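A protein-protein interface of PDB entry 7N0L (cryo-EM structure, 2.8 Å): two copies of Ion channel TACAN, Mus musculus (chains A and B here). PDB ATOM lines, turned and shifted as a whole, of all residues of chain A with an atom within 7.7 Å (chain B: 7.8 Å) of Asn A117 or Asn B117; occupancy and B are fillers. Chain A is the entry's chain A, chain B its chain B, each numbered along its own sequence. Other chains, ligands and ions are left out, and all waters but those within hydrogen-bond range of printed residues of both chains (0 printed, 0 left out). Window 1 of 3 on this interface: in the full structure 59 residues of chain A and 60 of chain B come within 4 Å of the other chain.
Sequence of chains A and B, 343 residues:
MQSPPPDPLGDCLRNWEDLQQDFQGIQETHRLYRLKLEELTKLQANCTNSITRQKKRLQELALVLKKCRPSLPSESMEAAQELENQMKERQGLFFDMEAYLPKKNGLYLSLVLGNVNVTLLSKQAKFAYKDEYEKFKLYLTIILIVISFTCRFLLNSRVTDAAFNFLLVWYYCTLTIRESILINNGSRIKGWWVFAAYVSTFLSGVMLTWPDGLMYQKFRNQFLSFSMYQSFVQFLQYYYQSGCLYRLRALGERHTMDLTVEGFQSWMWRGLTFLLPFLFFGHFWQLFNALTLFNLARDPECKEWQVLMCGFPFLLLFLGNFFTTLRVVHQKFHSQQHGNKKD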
ATOM      1  N   GLN A  44     -28.511  16.045  24.182  1.00  0.00           N
ATOM      2  CA  GLN A  44     -28.013  14.925  24.971  1.00  0.00           C
ATOM      3  C   GLN A  44     -27.885  15.307  26.437  1.00  0.00           C
ATOM      4  O   GLN A  44     -28.408  14.616  27.317  1.00  0.00           O
ATOM      5  CB  GLN A  44     -26.667  14.456  24.425  1.00  0.00           C
ATOM      6  CG  GLN A  44     -26.711  13.983  22.992  1.00  0.00           C
ATOM      7  CD  GLN A  44     -25.414  13.352  22.549  1.00  0.00           C
ATOM      8  OE1 GLN A  44     -24.337  13.891  22.788  1.00  0.00           O
ATOM      9  NE2 GLN A  44     -25.510  12.201  21.896  1.00  0.00           N
ATOM     10  N   LEU A 101     -27.858   7.729  25.272  1.00  0.00           N
ATOM     11  CA  LEU A 101     -27.130   8.899  25.740  1.00  0.00           C
ATOM     12  C   LEU A 101     -25.673   8.538  25.998  1.00  0.00           C
ATOM     13  O   LEU A 101     -25.383   7.431  26.458  1.00  0.00           O
ATOM     14  CB  LEU A 101     -27.738   9.454  27.022  1.00  0.00           C
ATOM     15  CG  LEU A 101     -29.050  10.229  26.951  1.00  0.00           C
ATOM     16  CD1 LEU A 101     -29.049  11.132  25.742  1.00  0.00           C
ATOM     17  CD2 LEU A 101     -30.240   9.304  26.936  1.00  0.00           C
ATOM     18  N   PRO A 102     -24.744   9.445  25.710  1.00  0.00           N
ATOM     19  CA  PRO A 102     -23.337   9.179  26.027  1.00  0.00           C
ATOM     20  C   PRO A 102     -23.123   9.136  27.532  1.00  0.00           C
ATOM     21  O   PRO A 102     -23.497  10.062  28.254  1.00  0.00           O
ATOM     22  CB  PRO A 102     -22.599  10.357  25.383  1.00  0.00           C
ATOM     23  CG  PRO A 102     -23.545  10.881  24.359  1.00  0.00           C
ATOM     24  CD  PRO A 102     -24.904  10.685  24.937  1.00  0.00           C
ATOM     25  N   LYS A 103     -22.524   8.047  28.001  1.00  0.00           N
ATOM     26  CA  LYS A 103     -22.155   7.910  29.402  1.00  0.00           C
ATOM     27  C   LYS A 103     -20.842   8.646  29.651  1.00  0.00           C
ATOM     28  O   LYS A 103     -20.352   9.403  28.810  1.00  0.00           O
ATOM     29  CB  LYS A 103     -22.046   6.439  29.792  1.00  0.00           C
ATOM     30  CG  LYS A 103     -23.364   5.748  30.045  1.00  0.00           C
ATOM     31  CD  LYS A 103     -23.152   4.463  30.827  1.00  0.00           C
ATOM     32  CE  LYS A 103     -24.435   3.660  30.940  1.00  0.00           C
ATOM     33  NZ  LYS A 103     -24.182   2.286  31.450  1.00  0.00           N
ATOM     34  N   LYS A 104     -20.255   8.425  30.822  1.00  0.00           N
ATOM     35  CA  LYS A 104     -18.931   8.931  31.139  1.00  0.00           C
ATOM     36  C   LYS A 104     -18.058   7.766  31.575  1.00  0.00           C
ATOM     37  O   LYS A 104     -18.520   6.866  32.280  1.00  0.00           O
ATOM     38  CB  LYS A 104     -18.994   9.999  32.233  1.00  0.00           C
ATOM     39  N   ASN A 105     -16.800   7.785  31.142  1.00  0.00           N
ATOM     40  CA  ASN A 105     -15.897   6.675  31.402  1.00  0.00           C
ATOM     41  C   ASN A 105     -15.744   6.436  32.899  1.00  0.00           C
ATOM     42  O   ASN A 105     -15.859   7.352  33.715  1.00  0.00           O
ATOM     43  CB  ASN A 105     -14.528   6.946  30.778  1.00  0.00           C
ATOM     44  CG  ASN A 105     -14.603   7.188  29.291  1.00  0.00           C
ATOM     45  OD1 ASN A 105     -15.654   7.016  28.677  1.00  0.00           O
ATOM     46  ND2 ASN A 105     -13.486   7.589  28.698  1.00  0.00           N
ATOM     47  N   LEU A 109     -11.296   3.461  32.274  1.00  0.00           N
ATOM     48  CA  LEU A 109     -11.220   4.002  30.923  1.00  0.00           C
ATOM     49  C   LEU A 109     -10.696   5.429  30.922  1.00  0.00           C
ATOM     50  O   LEU A 109      -9.995   5.826  29.988  1.00  0.00           O
ATOM     51  CB  LEU A 109     -12.584   3.935  30.243  1.00  0.00           C
ATOM     52  CG  LEU A 109     -12.983   2.596  29.623  1.00  0.00           C
ATOM     53  CD1 LEU A 109     -14.163   2.780  28.693  1.00  0.00           C
ATOM     54  CD2 LEU A 109     -11.816   1.967  28.883  1.00  0.00           C
ATOM     55  N   LEU A 113      -7.784   5.704  28.356  1.00  0.00           N
ATOM     56  CA  LEU A 113      -8.180   6.450  27.168  1.00  0.00           C
ATOM     57  C   LEU A 113      -8.285   7.948  27.393  1.00  0.00           C
ATOM     58  O   LEU A 113      -8.109   8.716  26.444  1.00  0.00           O
ATOM     59  CB  LEU A 113      -9.529   5.945  26.645  1.00  0.00           C
ATOM     60  CG  LEU A 113      -9.697   4.447  26.402  1.00  0.00           C
ATOM     61  CD1 LEU A 113     -10.948   4.189  25.591  1.00  0.00           C
ATOM     62  CD2 LEU A 113      -8.487   3.883  25.696  1.00  0.00           C
ATOM     63  N   GLY A 114      -8.562   8.383  28.615  1.00  0.00           N
ATOM     64  CA  GLY A 114      -8.867   9.776  28.850  1.00  0.00           C
ATOM     65  C   GLY A 114     -10.364   9.983  28.898  1.00  0.00           C
ATOM     66  O   GLY A 114     -11.101   9.065  29.261  1.00  0.00           O
ATOM     67  N   ASN A 115     -10.834  11.165  28.518  1.00  0.00           N
ATOM     68  CA  ASN A 115     -12.256  11.481  28.563  1.00  0.00           C
ATOM     69  C   ASN A 115     -12.866  11.532  27.166  1.00  0.00           C
ATOM     70  O   ASN A 115     -13.724  12.366  26.875  1.00  0.00           O
ATOM     71  CB  ASN A 115     -12.497  12.792  29.304  1.00  0.00           C
ATOM     72  CG  ASN A 115     -12.624  12.595  30.801  1.00  0.00           C
ATOM     73  OD1 ASN A 115     -11.964  13.272  31.587  1.00  0.00           O
ATOM     74  ND2 ASN A 115     -13.475  11.658  31.202  1.00  0.00           N
ATOM     75  N   VAL A 116     -12.419  10.639  26.282  1.00  0.00           N
ATOM     76  CA  VAL A 116     -13.141  10.428  25.037  1.00  0.00           C
ATOM     77  C   VAL A 116     -14.443   9.688  25.324  1.00  0.00           C
ATOM     78  O   VAL A 116     -14.626   9.063  26.375  1.00  0.00           O
ATOM     79  CB  VAL A 116     -12.283   9.660  24.021  1.00  0.00           C
ATOM     80  CG1 VAL A 116     -11.166  10.535  23.506  1.00  0.00           C
ATOM     81  CG2 VAL A 116     -11.729   8.395  24.646  1.00  0.00           C
ATOM     82  N   ASN A 117     -15.363   9.760  24.371  1.00  0.00           N
ATOM     83  CA  ASN A 117     -16.628   9.051  24.465  1.00  0.00           C
ATOM     84  C   ASN A 117     -16.508   7.729  23.722  1.00  0.00           C
ATOM     85  O   ASN A 117     -16.063   7.697  22.572  1.00  0.00           O
ATOM     86  CB  ASN A 117     -17.770   9.885  23.889  1.00  0.00           C
ATOM     87  CG  ASN A 117     -19.125   9.416  24.364  1.00  0.00           C
ATOM     88  OD1 ASN A 117     -19.941   8.934  23.579  1.00  0.00           O
ATOM     89  ND2 ASN A 117     -19.371   9.548  25.662  1.00  0.00           N
ATOM     90  N   VAL A 118     -16.902   6.643  24.382  1.00  0.00           N
ATOM     91  CA  VAL A 118     -16.779   5.302  23.828  1.00  0.00           C
ATOM     92  C   VAL A 118     -18.112   4.580  23.742  1.00  0.00           C
ATOM     93  O   VAL A 118     -18.140   3.400  23.381  1.00  0.00           O
ATOM     94  CB  VAL A 118     -15.772   4.455  24.630  1.00  0.00           C
ATOM     95  CG1 VAL A 118     -14.426   5.147  24.683  1.00  0.00           C
ATOM     96  CG2 VAL A 118     -16.295   4.200  26.027  1.00  0.00           C
ATOM     97  N   THR A 119     -19.216   5.243  24.064  1.00  0.00           N
ATOM     98  CA  THR A 119     -20.521   4.604  24.007  1.00  0.00           C
ATOM     99  C   THR A 119     -21.064   4.644  22.585  1.00  0.00           C
ATOM    100  O   THR A 119     -21.123   5.709  21.963  1.00  0.00           O
ATOM    101  CB  THR A 119     -21.496   5.291  24.959  1.00  0.00           C
ATOM    102  OG1 THR A 119     -21.906   6.540  24.395  1.00  0.00           O
ATOM    103  CG2 THR A 119     -20.838   5.541  26.303  1.00  0.00           C
ATOM    104  N   LEU A 120     -21.454   3.480  22.074  1.00  0.00           N
ATOM    105  CA  LEU A 120     -22.097   3.383  20.772  1.00  0.00           C
ATOM    106  C   LEU A 120     -23.566   3.741  20.930  1.00  0.00           C
ATOM    107  O   LEU A 120     -24.286   3.093  21.697  1.00  0.00           O
ATOM    108  CB  LEU A 120     -21.941   1.977  20.200  1.00  0.00           C
ATOM    109  CG  LEU A 120     -20.533   1.418  19.970  1.00  0.00           C
ATOM    110  CD1 LEU A 120     -19.567   2.506  19.530  1.00  0.00           C
ATOM    111  CD2 LEU A 120     -20.016   0.682  21.196  1.00  0.00           C
ATOM    112  N   LEU A 121     -24.015   4.766  20.207  1.00  0.00           N
ATOM    113  CA  LEU A 121     -25.333   5.350  20.424  1.00  0.00           C
ATOM    114  C   LEU A 121     -26.418   4.693  19.585  1.00  0.00           C
ATOM    115  O   LEU A 121     -27.459   5.309  19.328  1.00  0.00           O
ATOM    116  CB  LEU A 121     -25.283   6.854  20.154  1.00  0.00           C
ATOM    117  CG  LEU A 121     -24.991   7.766  21.347  1.00  0.00           C
ATOM    118  CD1 LEU A 121     -24.614   6.969  22.587  1.00  0.00           C
ATOM    119  CD2 LEU A 121     -23.897   8.754  21.002  1.00  0.00           C
ATOM    120  N   TYR A 129     -20.216  -3.964  17.688  1.00  0.00           N
ATOM    121  CA  TYR A 129     -19.015  -3.883  18.505  1.00  0.00           C
ATOM    122  C   TYR A 129     -18.826  -5.110  19.381  1.00  0.00           C
ATOM    123  O   TYR A 129     -17.686  -5.519  19.620  1.00  0.00           O
ATOM    124  CB  TYR A 129     -19.045  -2.626  19.375  1.00  0.00           C
ATOM    125  CG  TYR A 129     -17.817  -2.461  20.237  1.00  0.00           C
ATOM    126  CD1 TYR A 129     -17.835  -2.807  21.576  1.00  0.00           C
ATOM    127  CD2 TYR A 129     -16.636  -1.968  19.705  1.00  0.00           C
ATOM    128  CE1 TYR A 129     -16.716  -2.663  22.363  1.00  0.00           C
ATOM    129  CE2 TYR A 129     -15.513  -1.822  20.484  1.00  0.00           C
ATOM    130  CZ  TYR A 129     -15.560  -2.172  21.812  1.00  0.00           C
ATOM    131  OH  TYR A 129     -14.443  -2.026  22.593  1.00  0.00           O
ATOM    132  N   ILE A 181     -15.377  -1.022  27.602  1.00  0.00           N
ATOM    133  CA  ILE A 181     -16.201  -0.320  26.628  1.00  0.00           C
ATOM    134  C   ILE A 181     -17.528  -1.040  26.442  1.00  0.00           C
ATOM    135  O   ILE A 181     -18.538  -0.416  26.100  1.00  0.00           O
ATOM    136  CB  ILE A 181     -15.437  -0.173  25.302  1.00  0.00           C
ATOM    137  CG1 ILE A 181     -14.171   0.656  25.512  1.00  0.00           C
ATOM    138  CG2 ILE A 181     -16.305   0.475  24.243  1.00  0.00           C
ATOM    139  CD1 ILE A 181     -13.368   0.863  24.257  1.00  0.00           C
ATOM    140  N   ASN A 184     -19.994  -0.078  29.790  1.00  0.00           N
ATOM    141  CA  ASN A 184     -20.749   1.164  29.792  1.00  0.00           C
ATOM    142  C   ASN A 184     -21.672   1.297  28.590  1.00  0.00           C
ATOM    143  O   ASN A 184     -22.575   2.137  28.616  1.00  0.00           O
ATOM    144  CB  ASN A 184     -19.805   2.372  29.878  1.00  0.00           C
ATOM    145  CG  ASN A 184     -19.042   2.613  28.605  1.00  0.00           C
ATOM    146  OD1 ASN A 184     -18.811   1.698  27.824  1.00  0.00           O
ATOM    147  ND2 ASN A 184     -18.635   3.855  28.392  1.00  0.00           N
ATOM    148  N   GLN B  44     -23.602  13.316   9.001  1.00  0.00           N
ATOM    149  CA  GLN B  44     -22.164  13.095   9.079  1.00  0.00           C
ATOM    150  C   GLN B  44     -21.673  12.286   7.888  1.00  0.00           C
ATOM    151  O   GLN B  44     -20.734  12.690   7.196  1.00  0.00           O
ATOM    152  CB  GLN B  44     -21.809  12.389  10.385  1.00  0.00           C
ATOM    153  CG  GLN B  44     -22.222  13.139  11.627  1.00  0.00           C
ATOM    154  CD  GLN B  44     -21.664  12.526  12.888  1.00  0.00           C
ATOM    155  OE1 GLN B  44     -21.755  11.319  13.096  1.00  0.00           O
ATOM    156  NE2 GLN B  44     -21.081  13.358  13.741  1.00  0.00           N
ATOM    157  N   LEU B 101     -16.034  15.981  11.610  1.00  0.00           N
ATOM    158  CA  LEU B 101     -16.592  14.710  11.170  1.00  0.00           C
ATOM    159  C   LEU B 101     -15.891  13.559  11.879  1.00  0.00           C
ATOM    160  O   LEU B 101     -14.679  13.616  12.102  1.00  0.00           O
ATOM    161  CB  LEU B 101     -16.436  14.533   9.664  1.00  0.00           C
ATOM    162  CG  LEU B 101     -17.435  15.228   8.744  1.00  0.00           C
ATOM    163  CD1 LEU B 101     -18.820  15.166   9.341  1.00  0.00           C
ATOM    164  CD2 LEU B 101     -17.023  16.653   8.473  1.00  0.00           C
ATOM    165  N   PRO B 102     -16.624  12.512  12.248  1.00  0.00           N
ATOM    166  CA  PRO B 102     -15.978  11.347  12.862  1.00  0.00           C
ATOM    167  C   PRO B 102     -15.104  10.619  11.852  1.00  0.00           C
ATOM    168  O   PRO B 102     -15.557  10.255  10.765  1.00  0.00           O
ATOM    169  CB  PRO B 102     -17.159  10.483  13.315  1.00  0.00           C
ATOM    170  CG  PRO B 102     -18.313  11.425  13.384  1.00  0.00           C
ATOM    171  CD  PRO B 102     -18.090  12.405  12.285  1.00  0.00           C
ATOM    172  N   LYS B 103     -13.842  10.415  12.217  1.00  0.00           N
ATOM    173  CA  LYS B 103     -12.916   9.644  11.402  1.00  0.00           C
ATOM    174  C   LYS B 103     -13.144   8.157  11.651  1.00  0.00           C
ATOM    175  O   LYS B 103     -14.121   7.744  12.280  1.00  0.00           O
ATOM    176  CB  LYS B 103     -11.474  10.041  11.706  1.00  0.00           C
ATOM    177  CG  LYS B 103     -11.017  11.328  11.062  1.00  0.00           C
ATOM    178  CD  LYS B 103      -9.502  11.416  11.059  1.00  0.00           C
ATOM    179  CE  LYS B 103      -9.024  12.776  10.581  1.00  0.00           C
ATOM    180  NZ  LYS B 103      -7.571  12.972  10.839  1.00  0.00           N
ATOM    181  N   LYS B 104     -12.229   7.329  11.157  1.00  0.00           N
ATOM    182  CA  LYS B 104     -12.223   5.907  11.457  1.00  0.00           C
ATOM    183  C   LYS B 104     -10.858   5.533  12.008  1.00  0.00           C
ATOM    184  O   LYS B 104      -9.834   6.042  11.548  1.00  0.00           O
ATOM    185  CB  LYS B 104     -12.552   5.080  10.213  1.00  0.00           C
ATOM    186  N   ASN B 105     -10.854   4.650  13.004  1.00  0.00           N
ATOM    187  CA  ASN B 105      -9.622   4.292  13.689  1.00  0.00           C
ATOM    188  C   ASN B 105      -8.602   3.717  12.712  1.00  0.00           C
ATOM    189  O   ASN B 105      -8.950   3.118  11.692  1.00  0.00           O
ATOM    190  CB  ASN B 105      -9.906   3.279  14.797  1.00  0.00           C
ATOM    191  CG  ASN B 105     -10.917   3.781  15.801  1.00  0.00           C
ATOM    192  OD1 ASN B 105     -11.310   4.945  15.769  1.00  0.00           O
ATOM    193  ND2 ASN B 105     -11.343   2.907  16.701  1.00  0.00           N
ATOM    194  N   LEU B 109      -5.622   1.556  16.649  1.00  0.00           N
ATOM    195  CA  LEU B 109      -6.771   1.759  17.521  1.00  0.00           C
ATOM    196  C   LEU B 109      -7.849   0.715  17.275  1.00  0.00           C
ATOM    197  O   LEU B 109      -8.541   0.311  18.214  1.00  0.00           O
ATOM    198  CB  LEU B 109      -7.339   3.164  17.339  1.00  0.00           C
ATOM    199  CG  LEU B 109      -6.641   4.295  18.091  1.00  0.00           C
ATOM    200  CD1 LEU B 109      -7.510   5.533  18.103  1.00  0.00           C
ATOM    201  CD2 LEU B 109      -6.292   3.876  19.506  1.00  0.00           C
ATOM    202  N   LEU B 113      -8.884  -0.854  20.680  1.00  0.00           N
ATOM    203  CA  LEU B 113     -10.207  -0.410  21.099  1.00  0.00           C
ATOM    204  C   LEU B 113     -11.344  -1.050  20.322  1.00  0.00           C
ATOM    205  O   LEU B 113     -12.448  -1.173  20.857  1.00  0.00           O
ATOM    206  CB  LEU B 113     -10.328   1.112  20.965  1.00  0.00           C
ATOM    207  CG  LEU B 113      -9.253   1.984  21.612  1.00  0.00           C
ATOM    208  CD1 LEU B 113      -9.711   3.424  21.657  1.00  0.00           C
ATOM    209  CD2 LEU B 113      -8.933   1.490  23.003  1.00  0.00           C
ATOM    210  N   GLY B 114     -11.106  -1.460  19.083  1.00  0.00           N
ATOM    211  CA  GLY B 114     -12.189  -1.893  18.229  1.00  0.00           C
ATOM    212  C   GLY B 114     -12.617  -0.768  17.316  1.00  0.00           C
ATOM    213  O   GLY B 114     -11.807   0.100  16.984  1.00  0.00           O
ATOM    214  N   ASN B 115     -13.884  -0.745  16.921  1.00  0.00           N
ATOM    215  CA  ASN B 115     -14.390   0.272  16.008  1.00  0.00           C
ATOM    216  C   ASN B 115     -15.292   1.273  16.724  1.00  0.00           C
ATOM    217  O   ASN B 115     -16.299   1.727  16.179  1.00  0.00           O
ATOM    218  CB  ASN B 115     -15.123  -0.368  14.833  1.00  0.00           C
ATOM    219  CG  ASN B 115     -14.187  -0.735  13.700  1.00  0.00           C
ATOM    220  OD1 ASN B 115     -14.199  -1.861  13.206  1.00  0.00           O
ATOM    221  ND2 ASN B 115     -13.362   0.219  13.285  1.00  0.00           N
ATOM    222  N   VAL B 116     -14.942   1.618  17.963  1.00  0.00           N
ATOM    223  CA  VAL B 116     -15.569   2.763  18.602  1.00  0.00           C
ATOM    224  C   VAL B 116     -15.054   4.048  17.965  1.00  0.00           C
ATOM    225  O   VAL B 116     -14.013   4.078  17.298  1.00  0.00           O
ATOM    226  CB  VAL B 116     -15.319   2.761  20.118  1.00  0.00           C
ATOM    227  CG1 VAL B 116     -16.104   1.654  20.780  1.00  0.00           C
ATOM    228  CG2 VAL B 116     -13.838   2.614  20.406  1.00  0.00           C
ATOM    229  N   ASN B 117     -15.795   5.127  18.174  1.00  0.00           N
ATOM    230  CA  ASN B 117     -15.402   6.441  17.690  1.00  0.00           C
ATOM    231  C   ASN B 117     -14.686   7.184  18.808  1.00  0.00           C
ATOM    232  O   ASN B 117     -15.188   7.254  19.933  1.00  0.00           O
ATOM    233  CB  ASN B 117     -16.617   7.236  17.212  1.00  0.00           C
ATOM    234  CG  ASN B 117     -16.236   8.379  16.302  1.00  0.00           C
ATOM    235  OD1 ASN B 117     -16.413   9.548  16.646  1.00  0.00           O
ATOM    236  ND2 ASN B 117     -15.705   8.050  15.131  1.00  0.00           N
ATOM    237  N   VAL B 118     -13.514   7.734  18.497  1.00  0.00           N
ATOM    238  CA  VAL B 118     -12.675   8.397  19.483  1.00  0.00           C
ATOM    239  C   VAL B 118     -12.373   9.839  19.102  1.00  0.00           C
ATOM    240  O   VAL B 118     -11.575  10.496  19.767  1.00  0.00           O
ATOM    241  CB  VAL B 118     -11.368   7.614  19.716  1.00  0.00           C
ATOM    242  CG1 VAL B 118     -11.673   6.190  20.129  1.00  0.00           C
ATOM    243  CG2 VAL B 118     -10.514   7.637  18.467  1.00  0.00           C
ATOM    244  N   THR B 119     -12.992  10.346  18.042  1.00  0.00           N
ATOM    245  CA  THR B 119     -12.750  11.715  17.616  1.00  0.00           C
ATOM    246  C   THR B 119     -13.642  12.672  18.393  1.00  0.00           C
ATOM    247  O   THR B 119     -14.861  12.494  18.448  1.00  0.00           O
ATOM    248  CB  THR B 119     -13.002  11.863  16.117  1.00  0.00           C
ATOM    249  OG1 THR B 119     -14.411  11.855  15.873  1.00  0.00           O
ATOM    250  CG2 THR B 119     -12.355  10.724  15.356  1.00  0.00           C
ATOM    251  N   LEU B 120     -13.026  13.684  18.997  1.00  0.00           N
ATOM    252  CA  LEU B 120     -13.760  14.737  19.683  1.00  0.00           C
ATOM    253  C   LEU B 120     -14.252  15.737  18.648  1.00  0.00           C
ATOM    254  O   LEU B 120     -13.449  16.336  17.929  1.00  0.00           O
ATOM    255  CB  LEU B 120     -12.872  15.424  20.716  1.00  0.00           C
ATOM    256  CG  LEU B 120     -12.279  14.590  21.857  1.00  0.00           C
ATOM    257  CD1 LEU B 120     -13.230  13.489  22.298  1.00  0.00           C
ATOM    258  CD2 LEU B 120     -10.918  14.027  21.485  1.00  0.00           C
ATOM    259  N   LEU B 121     -15.568  15.921  18.572  1.00  0.00           N
ATOM    260  CA  LEU B 121     -16.184  16.674  17.490  1.00  0.00           C
ATOM    261  C   LEU B 121     -16.292  18.162  17.789  1.00  0.00           C
ATOM    262  O   LEU B 121     -17.114  18.852  17.177  1.00  0.00           O
ATOM    263  CB  LEU B 121     -17.563  16.095  17.173  1.00  0.00           C
ATOM    264  CG  LEU B 121     -17.631  15.018  16.089  1.00  0.00           C
ATOM    265  CD1 LEU B 121     -16.247  14.586  15.634  1.00  0.00           C
ATOM    266  CD2 LEU B 121     -18.420  13.823  16.581  1.00  0.00           C
ATOM    267  N   TYR B 129      -8.989  17.482  25.740  1.00  0.00           N
ATOM    268  CA  TYR B 129      -8.390  16.156  25.730  1.00  0.00           C
ATOM    269  C   TYR B 129      -6.874  16.206  25.621  1.00  0.00           C
ATOM    270  O   TYR B 129      -6.194  15.351  26.195  1.00  0.00           O
ATOM    271  CB  TYR B 129      -8.963  15.320  24.584  1.00  0.00           C
ATOM    272  CG  TYR B 129      -8.404  13.920  24.522  1.00  0.00           C
ATOM    273  CD1 TYR B 129      -7.406  13.591  23.622  1.00  0.00           C
ATOM    274  CD2 TYR B 129      -8.867  12.930  25.374  1.00  0.00           C
ATOM    275  CE1 TYR B 129      -6.890  12.318  23.566  1.00  0.00           C
ATOM    276  CE2 TYR B 129      -8.355  11.655  25.325  1.00  0.00           C
ATOM    277  CZ  TYR B 129      -7.368  11.356  24.419  1.00  0.00           C
ATOM    278  OH  TYR B 129      -6.857  10.085  24.366  1.00  0.00           O
ATOM    279  N   ILE B 181      -5.197   8.573  19.680  1.00  0.00           N
ATOM    280  CA  ILE B 181      -6.453   9.307  19.725  1.00  0.00           C
ATOM    281  C   ILE B 181      -6.214  10.779  19.423  1.00  0.00           C
ATOM    282  O   ILE B 181      -7.100  11.467  18.908  1.00  0.00           O
ATOM    283  CB  ILE B 181      -7.135   9.101  21.087  1.00  0.00           C
ATOM    284  CG1 ILE B 181      -7.465   7.626  21.296  1.00  0.00           C
ATOM    285  CG2 ILE B 181      -8.399   9.932  21.192  1.00  0.00           C
ATOM    286  CD1 ILE B 181      -8.152   7.337  22.602  1.00  0.00           C
ATOM    287  N   ASN B 184      -5.699  11.164  15.210  1.00  0.00           N
ATOM    288  CA  ASN B 184      -6.863  11.251  14.344  1.00  0.00           C
ATOM    289  C   ASN B 184      -7.790  12.399  14.717  1.00  0.00           C
ATOM    290  O   ASN B 184      -8.641  12.774  13.905  1.00  0.00           O
ATOM    291  CB  ASN B 184      -7.633   9.923  14.336  1.00  0.00           C
ATOM    292  CG  ASN B 184      -8.363   9.659  15.624  1.00  0.00           C
ATOM    293  OD1 ASN B 184      -7.980  10.150  16.680  1.00  0.00           O
ATOM    294  ND2 ASN B 184      -9.423   8.868  15.545  1.00  0.00           N
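The backbone carbonyl oxygen (O) of Leu A113 is in hydrogen-bond range of the side-chain hydroxyl (OH) of Tyr B129, at 2.8 Å. OH of Tyr A129 sits at hydrogen-bond distance from O of Leu B113 (2.8 Å). The backbone carbonyl oxygen (O) of Asn B117 sits close to the backbone carbonyl oxygen (O) of Asn A117 (2.8 Å).
The backbone carbonyl oxygen (O) of Lys A103 lies within hydrogen-bond range of the side-chain amide nitrogen (ND2) of Asn A117 (3.3 Å). The side-chain amide oxygen (OD1) of Asn A117 is in hydrogen-bond range of the side-chain hydroxyl (OG1) of Thr A119 (3.2 Å). The backbone carbonyl oxygen of Ile A181 lies close to the side-chain amide oxygen of Asn A184 (2.7 Å). The side-chain amide nitrogen of Asn B105 lies within hydrogen-bond range of the backbone carbonyl oxygen of Val B116 (3.0 Å). The side-chain amide oxygen (OD1) of Asn B117 sits at hydrogen-bond distance from the side-chain hydroxyl (OG1) of Thr B119. The backbone carbonyl oxygen of Ile B181 lies close to the side-chain amide oxygen of Asn B184.
Among the printed residues, merely in contact across the chains: Leu A113 with Leu B113, Val A116 with Val B118, Val A116 with Leu B120, Val A116 with Tyr B129, Val A116 with Ile B181, Val A118 with Val B116, Leu A120 with Val B116, Tyr A129 with Val B116 and Ile A181 with Val B116.
Asn A117 touches just one residue of chain B: Asn B117 (2.8 Å). Printed residues of chain B within 4 Å of Ile A181: Val B116. Of chain A, only Asn A117 comes within 4 Å of Asn B117. Of the printed residues of chain A, Tyr B129 touches Leu A113 and Val A116. The nearest residue of chain B that does not touch Asn A117 is Val B118 (4.6 Å). The nearest residue of chain A that does not touch Asn B117 is Val A118 (4.6 Å). The nearest printed residue of chain B that does not touch Val A116 is Asn B117 (5.6 Å).
Hydrophobic or aromatic side chains of chain B within 4 Å of the printed part of chain A: Leu B113, Val B116, Leu B120, Tyr B129 and Ile B181. Among the printed residues, 12 pairs touch across the chains. Among the printed residues, no Asp or Glu carboxylate lies within 4 Å of a Lys or Arg side-chain nitrogen of the other chain.
Leu B113 touches its own counterpart, Leu A113. Leu A113 touches Tyr B129, and with the chains exchanged Tyr A129 touches Leu B113. Val A116 touches Tyr B129, and with the chains exchanged Tyr A129 touches Val B116. Val A116 touches Ile B181, and with the chains exchanged Ile A181 touches Val B116. Positions printed for both chains: 44, 101, 102, 103, 104, 105, 109, 113, 114, 115, 116, 117, 118, 119, 120, 121, 129, 181 and 184.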
